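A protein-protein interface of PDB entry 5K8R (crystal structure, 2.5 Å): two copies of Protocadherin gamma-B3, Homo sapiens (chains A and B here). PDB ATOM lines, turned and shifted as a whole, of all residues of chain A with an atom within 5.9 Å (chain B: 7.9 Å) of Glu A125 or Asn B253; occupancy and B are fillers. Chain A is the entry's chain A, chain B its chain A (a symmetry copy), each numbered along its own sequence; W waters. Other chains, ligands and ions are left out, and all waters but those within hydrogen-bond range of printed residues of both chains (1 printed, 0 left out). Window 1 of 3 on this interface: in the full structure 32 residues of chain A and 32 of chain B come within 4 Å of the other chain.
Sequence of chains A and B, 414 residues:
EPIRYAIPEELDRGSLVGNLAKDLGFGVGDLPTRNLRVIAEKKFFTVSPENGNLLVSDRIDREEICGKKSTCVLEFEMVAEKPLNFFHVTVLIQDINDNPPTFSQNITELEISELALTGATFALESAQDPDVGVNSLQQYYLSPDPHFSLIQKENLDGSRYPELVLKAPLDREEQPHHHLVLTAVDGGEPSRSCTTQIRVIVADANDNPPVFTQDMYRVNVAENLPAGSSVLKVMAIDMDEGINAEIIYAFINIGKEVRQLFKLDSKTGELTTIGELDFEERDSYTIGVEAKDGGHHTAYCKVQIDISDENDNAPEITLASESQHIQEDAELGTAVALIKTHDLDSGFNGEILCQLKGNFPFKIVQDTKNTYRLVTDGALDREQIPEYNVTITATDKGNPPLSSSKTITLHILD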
ATOM      1  N   PHE A 103     -10.756  11.289   1.413  1.00  0.00           N
ATOM      2  CA  PHE A 103     -11.984  12.063   1.346  1.00  0.00           C
ATOM      3  C   PHE A 103     -13.065  11.390   2.183  1.00  0.00           C
ATOM      4  O   PHE A 103     -13.015  10.188   2.457  1.00  0.00           O
ATOM      5  CB  PHE A 103     -12.459  12.221  -0.101  1.00  0.00           C
ATOM      6  CG  PHE A 103     -11.636  13.184  -0.910  1.00  0.00           C
ATOM      7  CD1 PHE A 103     -10.636  12.726  -1.751  1.00  0.00           C
ATOM      8  CD2 PHE A 103     -11.866  14.548  -0.830  1.00  0.00           C
ATOM      9  CE1 PHE A 103      -9.880  13.612  -2.498  1.00  0.00           C
ATOM     10  CE2 PHE A 103     -11.114  15.438  -1.574  1.00  0.00           C
ATOM     11  CZ  PHE A 103     -10.119  14.970  -2.409  1.00  0.00           C
ATOM     12  N   SER A 104     -14.054  12.189   2.592  1.00  0.00           N
ATOM     13  CA  SER A 104     -15.109  11.668   3.457  1.00  0.00           C
ATOM     14  C   SER A 104     -15.942  10.610   2.743  1.00  0.00           C
ATOM     15  O   SER A 104     -16.317   9.597   3.343  1.00  0.00           O
ATOM     16  CB  SER A 104     -15.999  12.811   3.945  1.00  0.00           C
ATOM     17  OG  SER A 104     -15.251  13.754   4.690  1.00  0.00           O
ATOM     18  N   GLN A 105     -16.241  10.826   1.465  1.00  0.00           N
ATOM     19  CA  GLN A 105     -17.026   9.881   0.688  1.00  0.00           C
ATOM     20  C   GLN A 105     -16.445   9.767  -0.712  1.00  0.00           C
ATOM     21  O   GLN A 105     -15.847  10.712  -1.234  1.00  0.00           O
ATOM     22  CB  GLN A 105     -18.504  10.295   0.623  1.00  0.00           C
ATOM     23  CG  GLN A 105     -18.733  11.724   0.169  1.00  0.00           C
ATOM     24  CD  GLN A 105     -20.190  12.134   0.262  1.00  0.00           C
ATOM     25  OE1 GLN A 105     -21.026  11.381   0.760  1.00  0.00           O
ATOM     26  NE2 GLN A 105     -20.501  13.332  -0.218  1.00  0.00           N
ATOM     27  N   THR A 108     -19.582  12.401  -4.264  1.00  0.00           N
ATOM     28  CA  THR A 108     -20.251  13.554  -3.677  1.00  0.00           C
ATOM     29  C   THR A 108     -21.154  14.190  -4.725  1.00  0.00           C
ATOM     30  O   THR A 108     -20.717  14.446  -5.851  1.00  0.00           O
ATOM     31  CB  THR A 108     -19.239  14.585  -3.165  1.00  0.00           C
ATOM     32  OG1 THR A 108     -18.394  13.984  -2.174  1.00  0.00           O
ATOM     33  CG2 THR A 108     -19.956  15.784  -2.560  1.00  0.00           C
ATOM     34  N   ALA A 123     -17.761  25.573  -3.173  1.00  0.00           N
ATOM     35  CA  ALA A 123     -16.847  24.977  -2.211  1.00  0.00           C
ATOM     36  C   ALA A 123     -16.766  23.467  -2.398  1.00  0.00           C
ATOM     37  O   ALA A 123     -17.776  22.794  -2.617  1.00  0.00           O
ATOM     38  CB  ALA A 123     -17.292  25.303  -0.786  1.00  0.00           C
ATOM     39  N   LEU A 124     -15.549  22.938  -2.310  1.00  0.00           N
ATOM     40  CA  LEU A 124     -15.301  21.505  -2.372  1.00  0.00           C
ATOM     41  C   LEU A 124     -14.724  21.035  -1.046  1.00  0.00           C
ATOM     42  O   LEU A 124     -13.962  21.760  -0.397  1.00  0.00           O
ATOM     43  CB  LEU A 124     -14.343  21.152  -3.511  1.00  0.00           C
ATOM     44  CG  LEU A 124     -14.893  21.313  -4.926  1.00  0.00           C
ATOM     45  CD1 LEU A 124     -13.861  20.872  -5.951  1.00  0.00           C
ATOM     46  CD2 LEU A 124     -16.183  20.524  -5.077  1.00  0.00           C
ATOM     47  N   GLU A 125     -15.090  19.821  -0.645  1.00  0.00           N
ATOM     48  CA  GLU A 125     -14.559  19.259   0.588  1.00  0.00           C
ATOM     49  C   GLU A 125     -13.077  18.949   0.426  1.00  0.00           C
ATOM     50  O   GLU A 125     -12.665  18.316  -0.551  1.00  0.00           O
ATOM     51  CB  GLU A 125     -15.325  17.996   0.976  1.00  0.00           C
ATOM     52  CG  GLU A 125     -14.770  17.312   2.211  1.00  0.00           C
ATOM     53  CD  GLU A 125     -15.703  16.257   2.764  1.00  0.00           C
ATOM     54  OE1 GLU A 125     -16.533  15.727   1.994  1.00  0.00           O
ATOM     55  OE2 GLU A 125     -15.610  15.964   3.973  1.00  0.00           O
ATOM     56  N   SER A 126     -12.276  19.403   1.384  1.00  0.00           N
ATOM     57  CA  SER A 126     -10.844  19.166   1.342  1.00  0.00           C
ATOM     58  C   SER A 126     -10.518  17.755   1.825  1.00  0.00           C
ATOM     59  O   SER A 126     -11.311  17.102   2.510  1.00  0.00           O
ATOM     60  CB  SER A 126     -10.106  20.201   2.194  1.00  0.00           C
ATOM     61  OG  SER A 126      -8.703  20.035   2.097  1.00  0.00           O
ATOM     62  N   ALA A 127      -9.334  17.285   1.448  1.00  0.00           N
ATOM     63  CA  ALA A 127      -8.875  15.977   1.883  1.00  0.00           C
ATOM     64  C   ALA A 127      -8.235  16.071   3.265  1.00  0.00           C
ATOM     65  O   ALA A 127      -7.742  17.123   3.682  1.00  0.00           O
ATOM     66  CB  ALA A 127      -7.881  15.393   0.880  1.00  0.00           C
ATOM     67  N   GLN A 128      -8.252  14.949   3.980  1.00  0.00           N
ATOM     68  CA  GLN A 128      -7.665  14.860   5.308  1.00  0.00           C
ATOM     69  C   GLN A 128      -6.486  13.899   5.292  1.00  0.00           C
ATOM     70  O   GLN A 128      -6.465  12.925   4.533  1.00  0.00           O
ATOM     71  CB  GLN A 128      -8.697  14.407   6.347  1.00  0.00           C
ATOM     72  CG  GLN A 128      -9.802  15.418   6.596  1.00  0.00           C
ATOM     73  CD  GLN A 128     -10.695  15.031   7.756  1.00  0.00           C
ATOM     74  OE1 GLN A 128     -10.516  13.977   8.367  1.00  0.00           O
ATOM     75  NE2 GLN A 128     -11.661  15.886   8.070  1.00  0.00           N
ATOM     76  N   TYR A 140      -4.302  19.497  -4.986  1.00  0.00           N
ATOM     77  CA  TYR A 140      -5.535  19.025  -5.600  1.00  0.00           C
ATOM     78  C   TYR A 140      -5.494  19.221  -7.109  1.00  0.00           C
ATOM     79  O   TYR A 140      -4.996  20.237  -7.603  1.00  0.00           O
ATOM     80  CB  TYR A 140      -6.745  19.746  -5.007  1.00  0.00           C
ATOM     81  CG  TYR A 140      -6.916  19.501  -3.527  1.00  0.00           C
ATOM     82  CD1 TYR A 140      -7.618  18.396  -3.063  1.00  0.00           C
ATOM     83  CD2 TYR A 140      -6.366  20.367  -2.591  1.00  0.00           C
ATOM     84  CE1 TYR A 140      -7.772  18.165  -1.708  1.00  0.00           C
ATOM     85  CE2 TYR A 140      -6.514  20.143  -1.236  1.00  0.00           C
ATOM     86  CZ  TYR A 140      -7.218  19.041  -0.800  1.00  0.00           C
ATOM     87  OH  TYR A 140      -7.369  18.814   0.548  1.00  0.00           O
ATOM     88  N   PRO A 162      -9.389  23.208  -2.149  1.00  0.00           N
ATOM     89  CA  PRO A 162      -9.809  23.432  -3.535  1.00  0.00           C
ATOM     90  C   PRO A 162     -11.186  24.065  -3.649  1.00  0.00           C
ATOM     91  O   PRO A 162     -11.995  24.008  -2.716  1.00  0.00           O
ATOM     92  CB  PRO A 162      -9.802  22.016  -4.117  1.00  0.00           C
ATOM     93  CG  PRO A 162     -10.238  21.168  -2.952  1.00  0.00           C
ATOM     94  CD  PRO A 162      -9.725  21.848  -1.691  1.00  0.00           C
ATOM     95  N   LEU A 182     -11.670  14.263  -8.747  1.00  0.00           N
ATOM     96  CA  LEU A 182     -10.784  15.069  -7.958  1.00  0.00           C
ATOM     97  C   LEU A 182      -9.738  14.199  -7.315  1.00  0.00           C
ATOM     98  O   LEU A 182     -10.034  13.194  -6.748  1.00  0.00           O
ATOM     99  CB  LEU A 182     -11.584  15.772  -6.884  1.00  0.00           C
ATOM    100  CG  LEU A 182     -10.962  16.651  -5.831  1.00  0.00           C
ATOM    101  CD1 LEU A 182     -10.309  17.832  -6.475  1.00  0.00           C
ATOM    102  CD2 LEU A 182     -11.921  17.100  -4.783  1.00  0.00           C
ATOM    103  N   ALA B 250     -25.127  23.008   8.054  1.00  0.00           N
ATOM    104  CA  ALA B 250     -24.377  21.761   8.100  1.00  0.00           C
ATOM    105  C   ALA B 250     -22.904  22.063   8.325  1.00  0.00           C
ATOM    106  O   ALA B 250     -22.419  23.142   7.980  1.00  0.00           O
ATOM    107  CB  ALA B 250     -24.560  20.947   6.814  1.00  0.00           C
ATOM    108  N   PHE B 251     -22.203  21.098   8.911  1.00  0.00           N
ATOM    109  CA  PHE B 251     -20.757  21.186   9.044  1.00  0.00           C
ATOM    110  C   PHE B 251     -20.086  20.887   7.709  1.00  0.00           C
ATOM    111  O   PHE B 251     -20.626  20.165   6.866  1.00  0.00           O
ATOM    112  CB  PHE B 251     -20.252  20.210  10.107  1.00  0.00           C
ATOM    113  CG  PHE B 251     -20.573  20.620  11.517  1.00  0.00           C
ATOM    114  CD1 PHE B 251     -20.668  21.958  11.861  1.00  0.00           C
ATOM    115  CD2 PHE B 251     -20.775  19.665  12.499  1.00  0.00           C
ATOM    116  CE1 PHE B 251     -20.957  22.334  13.159  1.00  0.00           C
ATOM    117  CE2 PHE B 251     -21.066  20.035  13.797  1.00  0.00           C
ATOM    118  CZ  PHE B 251     -21.156  21.373  14.128  1.00  0.00           C
ATOM    119  N   ILE B 252     -18.896  21.458   7.516  1.00  0.00           N
ATOM    120  CA  ILE B 252     -18.092  21.194   6.331  1.00  0.00           C
ATOM    121  C   ILE B 252     -16.657  20.918   6.757  1.00  0.00           C
ATOM    122  O   ILE B 252     -16.180  21.431   7.774  1.00  0.00           O
ATOM    123  CB  ILE B 252     -18.138  22.359   5.316  1.00  0.00           C
ATOM    124  CG1 ILE B 252     -17.608  23.646   5.949  1.00  0.00           C
ATOM    125  CG2 ILE B 252     -19.551  22.556   4.783  1.00  0.00           C
ATOM    126  CD1 ILE B 252     -17.522  24.806   4.988  1.00  0.00           C
ATOM    127  N   ASN B 253     -15.972  20.090   5.964  1.00  0.00           N
ATOM    128  CA  ASN B 253     -14.570  19.735   6.202  1.00  0.00           C
ATOM    129  C   ASN B 253     -14.364  19.193   7.614  1.00  0.00           C
ATOM    130  O   ASN B 253     -13.349  19.453   8.263  1.00  0.00           O
ATOM    131  CB  ASN B 253     -13.649  20.928   5.937  1.00  0.00           C
ATOM    132  CG  ASN B 253     -13.613  21.321   4.475  1.00  0.00           C
ATOM    133  OD1 ASN B 253     -13.500  20.468   3.595  1.00  0.00           O
ATOM    134  ND2 ASN B 253     -13.714  22.618   4.207  1.00  0.00           N
ATOM    135  N   ILE B 254     -15.334  18.429   8.092  1.00  0.00           N
ATOM    136  CA  ILE B 254     -15.306  17.919   9.456  1.00  0.00           C
ATOM    137  C   ILE B 254     -14.632  16.556   9.468  1.00  0.00           C
ATOM    138  O   ILE B 254     -14.650  15.816   8.478  1.00  0.00           O
ATOM    139  CB  ILE B 254     -16.730  17.862  10.053  1.00  0.00           C
ATOM    140  CG1 ILE B 254     -16.666  18.015  11.570  1.00  0.00           C
ATOM    141  CG2 ILE B 254     -17.436  16.568   9.671  1.00  0.00           C
ATOM    142  CD1 ILE B 254     -15.903  19.240  12.005  1.00  0.00           C
ATOM    143  N   GLY B 255     -14.008  16.227  10.600  1.00  0.00           N
ATOM    144  CA  GLY B 255     -13.355  14.953  10.787  1.00  0.00           C
ATOM    145  C   GLY B 255     -14.162  14.042  11.701  1.00  0.00           C
ATOM    146  O   GLY B 255     -15.119  14.453  12.355  1.00  0.00           O
ATOM    147  N   LYS B 256     -13.748  12.772  11.733  1.00  0.00           N
ATOM    148  CA  LYS B 256     -14.456  11.795  12.552  1.00  0.00           C
ATOM    149  C   LYS B 256     -14.290  12.073  14.041  1.00  0.00           C
ATOM    150  O   LYS B 256     -15.178  11.734  14.831  1.00  0.00           O
ATOM    151  CB  LYS B 256     -13.984  10.382  12.217  1.00  0.00           C
ATOM    152  CG  LYS B 256     -14.550   9.841  10.915  1.00  0.00           C
ATOM    153  CD  LYS B 256     -14.313   8.347  10.790  1.00  0.00           C
ATOM    154  CE  LYS B 256     -15.034   7.779   9.579  1.00  0.00           C
ATOM    155  NZ  LYS B 256     -14.866   6.305   9.472  1.00  0.00           N
ATOM    156  N   VAL B 258     -14.437  14.942  15.350  1.00  0.00           N
ATOM    157  CA  VAL B 258     -15.377  16.012  15.660  1.00  0.00           C
ATOM    158  C   VAL B 258     -16.787  15.579  15.283  1.00  0.00           C
ATOM    159  O   VAL B 258     -17.767  16.022  15.893  1.00  0.00           O
ATOM    160  CB  VAL B 258     -14.985  17.310  14.935  1.00  0.00           C
ATOM    161  CG1 VAL B 258     -15.783  18.478  15.480  1.00  0.00           C
ATOM    162  CG2 VAL B 258     -13.487  17.554  15.070  1.00  0.00           C
ATOM    163  N   ARG B 259     -16.896  14.714  14.271  1.00  0.00           N
ATOM    164  CA  ARG B 259     -18.192  14.153  13.910  1.00  0.00           C
ATOM    165  C   ARG B 259     -18.808  13.385  15.074  1.00  0.00           C
ATOM    166  O   ARG B 259     -20.030  13.416  15.265  1.00  0.00           O
ATOM    167  CB  ARG B 259     -18.044  13.248  12.684  1.00  0.00           C
ATOM    168  CG  ARG B 259     -19.299  12.459  12.353  1.00  0.00           C
ATOM    169  CD  ARG B 259     -19.165  11.666  11.066  1.00  0.00           C
ATOM    170  NE  ARG B 259     -19.399  12.488   9.882  1.00  0.00           N
ATOM    171  CZ  ARG B 259     -18.435  13.051   9.162  1.00  0.00           C
ATOM    172  NH1 ARG B 259     -17.165  12.881   9.505  1.00  0.00           N
ATOM    173  NH2 ARG B 259     -18.738  13.781   8.098  1.00  0.00           N
ATOM    174  N   THR B 286     -12.065  24.454  15.541  1.00  0.00           N
ATOM    175  CA  THR B 286     -12.480  25.395  14.507  1.00  0.00           C
ATOM    176  C   THR B 286     -13.193  24.615  13.409  1.00  0.00           C
ATOM    177  O   THR B 286     -12.586  23.756  12.760  1.00  0.00           O
ATOM    178  CB  THR B 286     -11.288  26.166  13.941  1.00  0.00           C
ATOM    179  OG1 THR B 286     -10.735  27.008  14.962  1.00  0.00           O
ATOM    180  CG2 THR B 286     -11.724  27.029  12.767  1.00  0.00           C
ATOM    181  N   ILE B 287     -14.474  24.912  13.211  1.00  0.00           N
ATOM    182  CA  ILE B 287     -15.343  24.141  12.330  1.00  0.00           C
ATOM    183  C   ILE B 287     -16.004  25.086  11.338  1.00  0.00           C
ATOM    184  O   ILE B 287     -16.495  26.152  11.723  1.00  0.00           O
ATOM    185  CB  ILE B 287     -16.414  23.371  13.127  1.00  0.00           C
ATOM    186  CG1 ILE B 287     -15.761  22.491  14.195  1.00  0.00           C
ATOM    187  CG2 ILE B 287     -17.271  22.539  12.197  1.00  0.00           C
ATOM    188  CD1 ILE B 287     -16.739  21.960  15.219  1.00  0.00           C
ATOM    189  N   GLY B 288     -16.025  24.693  10.067  1.00  0.00           N
ATOM    190  CA  GLY B 288     -16.721  25.460   9.049  1.00  0.00           C
ATOM    191  C   GLY B 288     -18.194  25.082   8.984  1.00  0.00           C
ATOM    192  O   GLY B 288     -18.556  23.907   9.058  1.00  0.00           O
ATOM    193  N   VAL B 289     -19.041  26.096   8.832  1.00  0.00           N
ATOM    194  CA  VAL B 289     -20.489  25.927   8.810  1.00  0.00           C
ATOM    195  C   VAL B 289     -21.030  26.497   7.505  1.00  0.00           C
ATOM    196  O   VAL B 289     -20.659  27.608   7.104  1.00  0.00           O
ATOM    197  CB  VAL B 289     -21.158  26.601  10.022  1.00  0.00           C
ATOM    198  CG1 VAL B 289     -22.673  26.518   9.910  1.00  0.00           C
ATOM    199  CG2 VAL B 289     -20.681  25.954  11.314  1.00  0.00           C
ATOM    200  N   TYR B 300     -21.109  30.763   4.188  1.00  0.00           N
ATOM    201  CA  TYR B 300     -20.139  30.023   4.985  1.00  0.00           C
ATOM    202  C   TYR B 300     -19.625  30.888   6.123  1.00  0.00           C
ATOM    203  O   TYR B 300     -19.254  32.046   5.911  1.00  0.00           O
ATOM    204  CB  TYR B 300     -18.971  29.540   4.115  1.00  0.00           C
ATOM    205  CG  TYR B 300     -19.393  28.601   3.007  1.00  0.00           C
ATOM    206  CD1 TYR B 300     -19.799  29.090   1.772  1.00  0.00           C
ATOM    207  CD2 TYR B 300     -19.391  27.226   3.199  1.00  0.00           C
ATOM    208  CE1 TYR B 300     -20.189  28.236   0.758  1.00  0.00           C
ATOM    209  CE2 TYR B 300     -19.779  26.363   2.190  1.00  0.00           C
ATOM    210  CZ  TYR B 300     -20.178  26.874   0.972  1.00  0.00           C
ATOM    211  OH  TYR B 300     -20.565  26.020  -0.035  1.00  0.00           O
HETATM  212  O   HOH W   1     -12.506  23.095   1.335  1.00  0.00           O
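The backbone NH (N) of Ser A126 lies within hydrogen-bond range of the side-chain amide oxygen (OD1) of Asn B253.
The side-chain amide nitrogen (NE2) of Gln A128 lies within hydrogen-bond range of the backbone carbonyl oxygen (O) of Ile B254 (3.0 Å).
The side-chain amide nitrogen (NE2) of Gln A128 lies close to the backbone NH (N) of Gly B255.
Ala A123 touches Tyr B300 (CB to OH, 3.4 Å).
Glu A125 touches Asn B253 (CA to OD1, 3.4 Å).
Gln A128 touches Asn B253 (NE2 to O, 3.95 Å).
Gln A105 touches none of the printed residues of chain B.
Of the printed residues of chain B, Glu A125 touches Asn B253.
Of the printed residues of chain B, Ser A126 touches Asn B253.
Asn B253 touches just these residues of chain A: Glu A125, Ser A126 and Gln A128.
Of the printed residues of chain A, Gly B255 touches Gln A128 (3.3 Å).
Printed residues of chain A within 4 Å of Tyr B300: Ala A123 (3.4 Å).
The nearest residue of chain A that does not touch Asn B253 is Leu A124 (4.2 Å).
Of the 14 printed residues of chain B, 4 touch a printed residue of chain A.
Among the printed residues, no Asp or Glu carboxylate lies within 4 Å of a Lys or Arg side-chain nitrogen of the other chain.
No position is printed for both chains.
Water W1 lies within hydrogen-bond range of O of Leu A124 (2.6 Å) and ND2 of Asn B253 (3.2 Å).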
